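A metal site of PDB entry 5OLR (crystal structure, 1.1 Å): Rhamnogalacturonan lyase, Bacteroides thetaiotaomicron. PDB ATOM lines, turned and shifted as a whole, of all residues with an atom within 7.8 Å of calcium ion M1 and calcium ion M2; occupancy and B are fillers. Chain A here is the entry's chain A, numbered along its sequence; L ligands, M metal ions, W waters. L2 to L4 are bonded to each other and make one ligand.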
ATOM      1  N   ILE A 160     -16.582  -9.003 -23.465  1.00  0.00           N
ATOM      2  CA  ILE A 160     -17.955  -8.552 -23.495  1.00  0.00           C
ATOM      3  C   ILE A 160     -18.791  -9.605 -24.205  1.00  0.00           C
ATOM      4  O   ILE A 160     -18.326 -10.202 -25.181  1.00  0.00           O
ATOM      5  CB  ILE A 160     -18.029  -7.216 -24.288  1.00  0.00           C
ATOM      6  CG1 ILE A 160     -17.179  -6.117 -23.624  1.00  0.00           C
ATOM      7  CG2 ILE A 160     -19.442  -6.768 -24.486  1.00  0.00           C
ATOM      8  CD1 ILE A 160     -16.692  -5.071 -24.599  1.00  0.00           C
ATOM      9  N   GLY A 190     -11.011  -4.769 -14.861  1.00  0.00           N
ATOM     10  CA  GLY A 190     -12.213  -5.339 -15.474  1.00  0.00           C
ATOM     11  C   GLY A 190     -13.283  -4.334 -15.864  1.00  0.00           C
ATOM     12  O   GLY A 190     -14.446  -4.687 -16.073  1.00  0.00           O
ATOM     13  N   GLY A 191     -12.916  -3.055 -16.019  1.00  0.00           N
ATOM     14  CA  GLY A 191     -13.879  -1.994 -16.242  1.00  0.00           C
ATOM     15  C   GLY A 191     -14.476  -1.866 -17.610  1.00  0.00           C
ATOM     16  O   GLY A 191     -15.299  -0.966 -17.797  1.00  0.00           O
ATOM     17  N   ASN A 192     -14.124  -2.731 -18.560  1.00  0.00           N
ATOM     18  CA  ASN A 192     -14.739  -2.671 -19.878  1.00  0.00           C
ATOM     19  C   ASN A 192     -15.540  -3.907 -20.220  1.00  0.00           C
ATOM     20  O   ASN A 192     -16.017  -4.010 -21.335  1.00  0.00           O
ATOM     21  CB  ASN A 192     -13.682  -2.412 -20.956  1.00  0.00           C
ATOM     22  CG  ASN A 192     -12.945  -1.110 -20.738  1.00  0.00           C
ATOM     23  OD1 ASN A 192     -13.534  -0.106 -20.363  1.00  0.00           O
ATOM     24  ND2 ASN A 192     -11.647  -1.145 -20.887  1.00  0.00           N
ATOM     25  N   VAL A 193     -15.698  -4.832 -19.269  1.00  0.00           N
ATOM     26  CA  VAL A 193     -16.425  -6.087 -19.566  1.00  0.00           C
ATOM     27  C   VAL A 193     -17.873  -6.021 -19.075  1.00  0.00           C
ATOM     28  O   VAL A 193     -18.137  -6.183 -17.899  1.00  0.00           O
ATOM     29  CB  VAL A 193     -15.709  -7.306 -19.026  1.00  0.00           C
ATOM     30  CG1 VAL A 193     -16.411  -8.582 -19.513  1.00  0.00           C
ATOM     31  CG2 VAL A 193     -14.264  -7.322 -19.443  1.00  0.00           C
ATOM     32  N   ASP A 194     -18.797  -5.787 -20.015  1.00  0.00           N
ATOM     33  CA  ASP A 194     -20.207  -5.827 -19.769  1.00  0.00           C
ATOM     34  C   ASP A 194     -20.779  -7.137 -20.339  1.00  0.00           C
ATOM     35  O   ASP A 194     -20.219  -7.693 -21.275  1.00  0.00           O
ATOM     36  CB  ASP A 194     -20.917  -4.649 -20.468  1.00  0.00           C
ATOM     37  CG  ASP A 194     -20.529  -3.281 -19.949  1.00  0.00           C
ATOM     38  OD1 ASP A 194     -20.161  -3.170 -18.750  1.00  0.00           O
ATOM     39  OD2 ASP A 194     -20.653  -2.305 -20.692  1.00  0.00           O
ATOM     40  N   GLY A 195     -21.920  -7.551 -19.825  1.00  0.00           N
ATOM     41  CA  GLY A 195     -22.647  -8.661 -20.432  1.00  0.00           C
ATOM     42  C   GLY A 195     -23.157  -8.270 -21.812  1.00  0.00           C
ATOM     43  O   GLY A 195     -22.878  -8.973 -22.800  1.00  0.00           O
ATOM     44  N   PHE A 196     -23.904  -7.157 -21.857  1.00  0.00           N
ATOM     45  CA  PHE A 196     -24.611  -6.701 -23.040  1.00  0.00           C
ATOM     46  C   PHE A 196     -24.428  -5.214 -23.208  1.00  0.00           C
ATOM     47  O   PHE A 196     -24.701  -4.443 -22.262  1.00  0.00           O
ATOM     48  CB  PHE A 196     -26.103  -6.996 -22.876  1.00  0.00           C
ATOM     49  CG  PHE A 196     -26.417  -8.472 -22.672  1.00  0.00           C
ATOM     50  CD1 PHE A 196     -26.428  -9.031 -21.418  1.00  0.00           C
ATOM     51  CD2 PHE A 196     -26.709  -9.287 -23.757  1.00  0.00           C
ATOM     52  CE1 PHE A 196     -26.693 -10.391 -21.242  1.00  0.00           C
ATOM     53  CE2 PHE A 196     -26.992 -10.630 -23.578  1.00  0.00           C
ATOM     54  CZ  PHE A 196     -26.966 -11.168 -22.329  1.00  0.00           C
ATOM     55  N   GLY A 197     -23.954  -4.806 -24.370  1.00  0.00           N
ATOM     56  CA  GLY A 197     -23.675  -3.411 -24.675  1.00  0.00           C
ATOM     57  C   GLY A 197     -24.416  -2.955 -25.898  1.00  0.00           C
ATOM     58  O   GLY A 197     -24.290  -3.549 -26.980  1.00  0.00           O
ATOM     59  N   HIS A 199     -24.573   0.300 -28.178  1.00  0.00           N
ATOM     60  CA  HIS A 199     -23.772   1.521 -28.423  1.00  0.00           C
ATOM     61  C   HIS A 199     -23.821   1.879 -29.911  1.00  0.00           C
ATOM     62  O   HIS A 199     -22.801   2.079 -30.557  1.00  0.00           O
ATOM     63  CB  HIS A 199     -22.321   1.334 -27.945  1.00  0.00           C
ATOM     64  CG  HIS A 199     -22.184   0.665 -26.631  1.00  0.00           C
ATOM     65  ND1 HIS A 199     -22.550   1.262 -25.448  1.00  0.00           N
ATOM     66  CD2 HIS A 199     -21.675  -0.548 -26.307  1.00  0.00           C
ATOM     67  CE1 HIS A 199     -22.273   0.433 -24.457  1.00  0.00           C
ATOM     68  NE2 HIS A 199     -21.741  -0.674 -24.945  1.00  0.00           N
ATOM     69  N   SER A 224     -17.649  -8.172 -14.960  1.00  0.00           N
ATOM     70  CA  SER A 224     -16.837  -7.352 -14.078  1.00  0.00           C
ATOM     71  C   SER A 224     -17.209  -5.878 -14.073  1.00  0.00           C
ATOM     72  O   SER A 224     -16.996  -5.217 -13.067  1.00  0.00           O
ATOM     73  CB  SER A 224     -15.354  -7.585 -14.341  1.00  0.00           C
ATOM     74  OG  SER A 224     -14.969  -7.355 -15.696  1.00  0.00           O
ATOM     75  N   ASP A 225     -17.803  -5.371 -15.159  1.00  0.00           N
ATOM     76  CA  ASP A 225     -18.238  -4.000 -15.184  1.00  0.00           C
ATOM     77  C   ASP A 225     -19.733  -3.936 -14.927  1.00  0.00           C
ATOM     78  O   ASP A 225     -20.155  -3.966 -13.755  1.00  0.00           O
ATOM     79  CB  ASP A 225     -17.734  -3.282 -16.476  1.00  0.00           C
ATOM     80  CG  ASP A 225     -17.728  -1.785 -16.391  1.00  0.00           C
ATOM     81  OD1 ASP A 225     -17.173  -1.252 -15.383  1.00  0.00           O
ATOM     82  OD2 ASP A 225     -18.192  -1.106 -17.313  1.00  0.00           O
ATOM     83  N   ASP A 226     -20.558  -3.834 -15.996  1.00  0.00           N
ATOM     84  CA  ASP A 226     -22.028  -3.732 -15.875  1.00  0.00           C
ATOM     85  C   ASP A 226     -22.706  -4.952 -16.470  1.00  0.00           C
ATOM     86  O   ASP A 226     -22.151  -5.606 -17.358  1.00  0.00           O
ATOM     87  CB  ASP A 226     -22.493  -2.469 -16.595  1.00  0.00           C
ATOM     88  CG  ASP A 226     -21.792  -1.218 -16.115  1.00  0.00           C
ATOM     89  OD1 ASP A 226     -21.782  -0.953 -14.885  1.00  0.00           O
ATOM     90  OD2 ASP A 226     -21.260  -0.473 -16.972  1.00  0.00           O
ATOM     91  N   GLY A 227     -23.938  -5.207 -16.062  1.00  0.00           N
ATOM     92  CA  GLY A 227     -24.691  -6.229 -16.755  1.00  0.00           C
ATOM     93  C   GLY A 227     -25.099  -5.802 -18.164  1.00  0.00           C
ATOM     94  O   GLY A 227     -24.823  -6.504 -19.143  1.00  0.00           O
ATOM     95  N   PHE A 228     -25.757  -4.648 -18.245  1.00  0.00           N
ATOM     96  CA  PHE A 228     -26.270  -4.060 -19.492  1.00  0.00           C
ATOM     97  C   PHE A 228     -25.825  -2.585 -19.491  1.00  0.00           C
ATOM     98  O   PHE A 228     -25.927  -1.903 -18.471  1.00  0.00           O
ATOM     99  CB  PHE A 228     -27.806  -4.083 -19.557  1.00  0.00           C
ATOM    100  CG  PHE A 228     -28.389  -5.471 -19.632  1.00  0.00           C
ATOM    101  CD1 PHE A 228     -28.486  -6.253 -18.500  1.00  0.00           C
ATOM    102  CD2 PHE A 228     -28.818  -6.002 -20.827  1.00  0.00           C
ATOM    103  CE1 PHE A 228     -29.013  -7.565 -18.563  1.00  0.00           C
ATOM    104  CE2 PHE A 228     -29.348  -7.274 -20.897  1.00  0.00           C
ATOM    105  CZ  PHE A 228     -29.412  -8.048 -19.779  1.00  0.00           C
ATOM    106  N   ASP A 229     -25.368  -2.106 -20.648  1.00  0.00           N
ATOM    107  CA  ASP A 229     -24.829  -0.744 -20.781  1.00  0.00           C
ATOM    108  C   ASP A 229     -25.200  -0.184 -22.140  1.00  0.00           C
ATOM    109  O   ASP A 229     -24.846  -0.777 -23.169  1.00  0.00           O
ATOM    110  CB  ASP A 229     -23.316  -0.829 -20.524  1.00  0.00           C
ATOM    111  CG  ASP A 229     -22.570   0.478 -20.662  1.00  0.00           C
ATOM    112  OD1 ASP A 229     -22.965   1.350 -21.431  1.00  0.00           O
ATOM    113  OD2 ASP A 229     -21.476   0.567 -20.016  1.00  0.00           O
ATOM    114  N   LEU A 230     -25.887   0.957 -22.111  1.00  0.00           N
ATOM    115  CA  LEU A 230     -26.372   1.667 -23.298  1.00  0.00           C
ATOM    116  C   LEU A 230     -25.701   3.035 -23.447  1.00  0.00           C
ATOM    117  O   LEU A 230     -26.283   3.933 -24.051  1.00  0.00           O
ATOM    118  CB  LEU A 230     -27.897   1.865 -23.240  1.00  0.00           C
ATOM    119  CG  LEU A 230     -28.736   0.598 -23.040  1.00  0.00           C
ATOM    120  CD1 LEU A 230     -30.211   0.948 -23.080  1.00  0.00           C
ATOM    121  CD2 LEU A 230     -28.426  -0.478 -24.080  1.00  0.00           C
ATOM    122  N   ILE A 231     -24.462   3.211 -22.975  1.00  0.00           N
ATOM    123  CA  ILE A 231     -23.795   4.507 -23.186  1.00  0.00           C
ATOM    124  C   ILE A 231     -23.523   4.739 -24.678  1.00  0.00           C
ATOM    125  O   ILE A 231     -23.331   3.826 -25.454  1.00  0.00           O
ATOM    126  CB  ILE A 231     -22.463   4.588 -22.367  1.00  0.00           C
ATOM    127  CG1 ILE A 231     -22.094   6.035 -22.056  1.00  0.00           C
ATOM    128  CG2 ILE A 231     -21.338   3.829 -23.037  1.00  0.00           C
ATOM    129  CD1 ILE A 231     -20.864   6.177 -21.171  1.00  0.00           C
ATOM    130  N   GLY A 258     -15.253  -3.681 -11.632  1.00  0.00           N
ATOM    131  CA  GLY A 258     -15.691  -2.485 -12.311  1.00  0.00           C
ATOM    132  C   GLY A 258     -16.905  -1.820 -11.724  1.00  0.00           C
ATOM    133  O   GLY A 258     -17.177  -1.900 -10.554  1.00  0.00           O
ATOM    134  N   ASP A 259     -17.658  -1.180 -12.604  1.00  0.00           N
ATOM    135  CA  ASP A 259     -18.638  -0.187 -12.209  1.00  0.00           C
ATOM    136  C   ASP A 259     -19.867  -0.746 -11.484  1.00  0.00           C
ATOM    137  O   ASP A 259     -20.487  -0.041 -10.685  1.00  0.00           O
ATOM    138  CB  ASP A 259     -19.079   0.609 -13.451  1.00  0.00           C
ATOM    139  CG  ASP A 259     -17.970   1.459 -14.082  1.00  0.00           C
ATOM    140  OD1 ASP A 259     -17.069   1.891 -13.339  1.00  0.00           O
ATOM    141  OD2 ASP A 259     -17.972   1.741 -15.343  1.00  0.00           O
ATOM    142  N   GLY A 260     -20.274  -1.992 -11.767  1.00  0.00           N
ATOM    143  CA  GLY A 260     -21.335  -2.615 -10.994  1.00  0.00           C
ATOM    144  C   GLY A 260     -22.706  -2.004 -11.115  1.00  0.00           C
ATOM    145  O   GLY A 260     -23.403  -1.859 -10.091  1.00  0.00           O
ATOM    146  N   THR A 261     -23.116  -1.720 -12.363  1.00  0.00           N
ATOM    147  CA  THR A 261     -24.486  -1.327 -12.613  1.00  0.00           C
ATOM    148  C   THR A 261     -25.257  -2.514 -13.134  1.00  0.00           C
ATOM    149  O   THR A 261     -24.767  -3.231 -14.019  1.00  0.00           O
ATOM    150  CB  THR A 261     -24.592  -0.214 -13.681  1.00  0.00           C
ATOM    151  OG1 THR A 261     -23.487   0.658 -13.611  1.00  0.00           O
ATOM    152  CG2 THR A 261     -25.893   0.552 -13.588  1.00  0.00           C
ATOM    153  N   LYS A 264     -27.235   0.159 -16.997  1.00  0.00           N
ATOM    154  CA  LYS A 264     -26.677   1.491 -17.266  1.00  0.00           C
ATOM    155  C   LYS A 264     -27.356   1.912 -18.571  1.00  0.00           C
ATOM    156  O   LYS A 264     -26.985   1.461 -19.621  1.00  0.00           O
ATOM    157  CB  LYS A 264     -25.147   1.383 -17.359  1.00  0.00           C
ATOM    158  CG  LYS A 264     -24.460   2.680 -17.712  1.00  0.00           C
ATOM    159  CD  LYS A 264     -22.950   2.543 -17.605  1.00  0.00           C
ATOM    160  CE  LYS A 264     -22.446   2.661 -16.180  1.00  0.00           C
ATOM    161  NZ  LYS A 264     -21.016   2.232 -16.097  1.00  0.00           N
ATOM    162  N   ASN A 303     -27.420   7.217 -15.934  1.00  0.00           N
ATOM    163  CA  ASN A 303     -26.055   7.374 -16.382  1.00  0.00           C
ATOM    164  C   ASN A 303     -25.793   8.682 -17.118  1.00  0.00           C
ATOM    165  O   ASN A 303     -25.075   8.692 -18.110  1.00  0.00           O
ATOM    166  CB  ASN A 303     -25.616   6.172 -17.238  1.00  0.00           C
ATOM    167  CG  ASN A 303     -24.119   6.124 -17.434  1.00  0.00           C
ATOM    168  OD1 ASN A 303     -23.392   6.319 -16.477  1.00  0.00           O
ATOM    169  ND2 ASN A 303     -23.654   5.864 -18.649  1.00  0.00           N
HETATM  170  P1  LIG L   1     -19.049   2.851 -19.080  1.00  0.00           P
HETATM  171  O1  LIG L   1     -19.551   3.734 -17.922  1.00  0.00           O
HETATM  172  O2  LIG L   1     -17.829   3.523 -19.659  1.00  0.00           O
HETATM  173  O3  LIG L   1     -20.142   2.824 -20.148  1.00  0.00           O
HETATM  174  O4  LIG L   1     -18.807   1.477 -18.550  1.00  0.00           O
HETATM  175  C1  LG2 L   2     -16.373   3.332 -22.958  1.00  0.00           C
HETATM  176  C2  LG2 L   2     -15.230   2.847 -23.839  1.00  0.00           C
HETATM  177  C3  LG2 L   2     -15.198   1.309 -23.876  1.00  0.00           C
HETATM  178  C4  LG2 L   2     -16.545   0.777 -24.335  1.00  0.00           C
HETATM  179  C5  LG2 L   2     -17.621   1.302 -23.379  1.00  0.00           C
HETATM  180  C6  LG2 L   2     -19.027   0.888 -23.771  1.00  0.00           C
HETATM  181  O1  LG2 L   2     -16.114   3.014 -21.609  1.00  0.00           O
HETATM  182  O2  LG2 L   2     -15.539   3.332 -25.148  1.00  0.00           O
HETATM  183  O3  LG2 L   2     -14.110   0.885 -24.709  1.00  0.00           O
HETATM  184  O4  LG2 L   2     -16.546  -0.646 -24.264  1.00  0.00           O
HETATM  185  O5  LG2 L   2     -17.596   2.723 -23.402  1.00  0.00           O
HETATM  186  C1  LG3 L   3     -14.565   4.112 -25.836  1.00  0.00           C
HETATM  187  C2  LG3 L   3     -15.277   4.946 -26.896  1.00  0.00           C
HETATM  188  C3  LG3 L   3     -15.787   4.056 -27.997  1.00  0.00           C
HETATM  189  C4  LG3 L   3     -14.667   3.172 -28.520  1.00  0.00           C
HETATM  190  C5  LG3 L   3     -14.052   2.373 -27.376  1.00  0.00           C
HETATM  191  C6  LG3 L   3     -12.966   1.438 -27.805  1.00  0.00           C
HETATM  192  O1  LG3 L   3     -16.375   5.642 -26.292  1.00  0.00           O
HETATM  193  O2  LG3 L   3     -16.361   4.856 -29.024  1.00  0.00           O
HETATM  194  O3  LG3 L   3     -13.638   3.950 -29.160  1.00  0.00           O
HETATM  195  O4  LG3 L   3     -13.528   3.290 -26.392  1.00  0.00           O
HETATM  196  O5  LG3 L   3     -13.311   0.505 -28.578  1.00  0.00           O
HETATM  197  O6  LG3 L   3     -11.789   1.596 -27.368  1.00  0.00           O
HETATM  198  C1  LG4 L   4     -13.756   4.063 -30.550  1.00  0.00           C
HETATM  199  C2  LG4 L   4     -12.971   5.251 -31.025  1.00  0.00           C
HETATM  200  C3  LG4 L   4     -11.495   4.897 -30.879  1.00  0.00           C
HETATM  201  C4  LG4 L   4     -11.173   3.561 -31.565  1.00  0.00           C
HETATM  202  C5  LG4 L   4     -12.092   2.441 -31.044  1.00  0.00           C
HETATM  203  C6  LG4 L   4     -11.898   1.127 -31.780  1.00  0.00           C
HETATM  204  O1  LG4 L   4     -13.289   5.478 -32.396  1.00  0.00           O
HETATM  205  O2  LG4 L   4     -10.676   5.931 -31.444  1.00  0.00           O
HETATM  206  O3  LG4 L   4      -9.839   3.194 -31.297  1.00  0.00           O
HETATM  207  O4  LG4 L   4     -13.437   2.864 -31.208  1.00  0.00           O
HETATM  208 CA    CA M   1     -19.853  -0.695 -18.900  1.00  0.00          CA
HETATM  209 CA    CA M   2     -16.815   0.790 -17.264  1.00  0.00          CA
HETATM  210  O   HOH W   1     -14.872   1.184 -15.720  1.00  0.00           O
HETATM  211  O   HOH W   2     -16.001   0.793 -19.828  1.00  0.00           O
HETATM  212  O   HOH W   3     -18.108  -0.871 -20.448  1.00  0.00           O
HETATM  213  O   HOH W   4     -15.975   3.086 -17.709  1.00  0.00           O
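N of Asp 225 is in hydrogen-bond range of O of Val 193. N of Gly 260 lies within hydrogen-bond range of O of Asp 225, 2.8 Å away. The backbone NH of Ile 231 is in hydrogen-bond range of the side-chain carboxylate of Asp 229. The backbone NH (N) of Asp 229 lies within hydrogen-bond range of the backbone carbonyl oxygen (O) of Phe 196 (2.9 Å). The side-chain amino group of Lys 264 is in salt-bridge range of the side-chain carboxylate of Asp 226. OD1 of Asp 226 is in hydrogen-bond range of OG1 of Thr 261, 2.7 Å away. N of Gly 195 is in hydrogen-bond range of O of Asp 226 (3.1 Å). OD2 of Asp 259 lies close to NZ of Lys 264, 3.2 Å away.
Four residues have an atom within 4 Å of calcium ion M1: Asp 194, Asp 225, Asp 226 and Asp 229. The nearest printed residue that does not touch calcium ion M1 is Lys 264 (4.2 Å).
Of the 24 residues printed, 3 come within 4 Å of calcium ion M2.
Calcium ion M1 is bound by the side-chain carboxylate (OD2) of Asp 225 (2.3 Å), water W3 (2.3 Å), the side-chain carboxylate (OD2) of Asp 229 (2.3 Å), the side-chain carboxylate (OD2) of Asp 226 (2.4 Å), an oxygen (O4) of LIG L1 (2.4 Å), the side-chain carboxylate (OD1) of Asp 194 (2.5 Å) and the side-chain carboxylate (OD2) of Asp 194 (2.5 Å).
The side-chain carboxylate (OD2) of Asp 225 is bound to calcium ion M2, 2.3 Å away. O of Gly 191 binds calcium ion M2 (2.4 Å). OD2 of Asp 259 is bound to calcium ion M2 (2.4 Å). Calcium ion M2 is bound by O4 of LIG L1 (2.5 Å). Water W4 binds calcium ion M2, at 2.5 Å. Water W1 is bound to calcium ion M2. Water W2 is bound to calcium ion M2 (2.7 Å). Calcium ion M2 is bound by the side-chain carboxylate (OD1) of Asp 225 (2.8 Å).
Water W2 bridges the side-chain amide oxygen of Asn 192 (2.7 Å) and an oxygen (O1) of LG2 L2 (2.8 Å).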
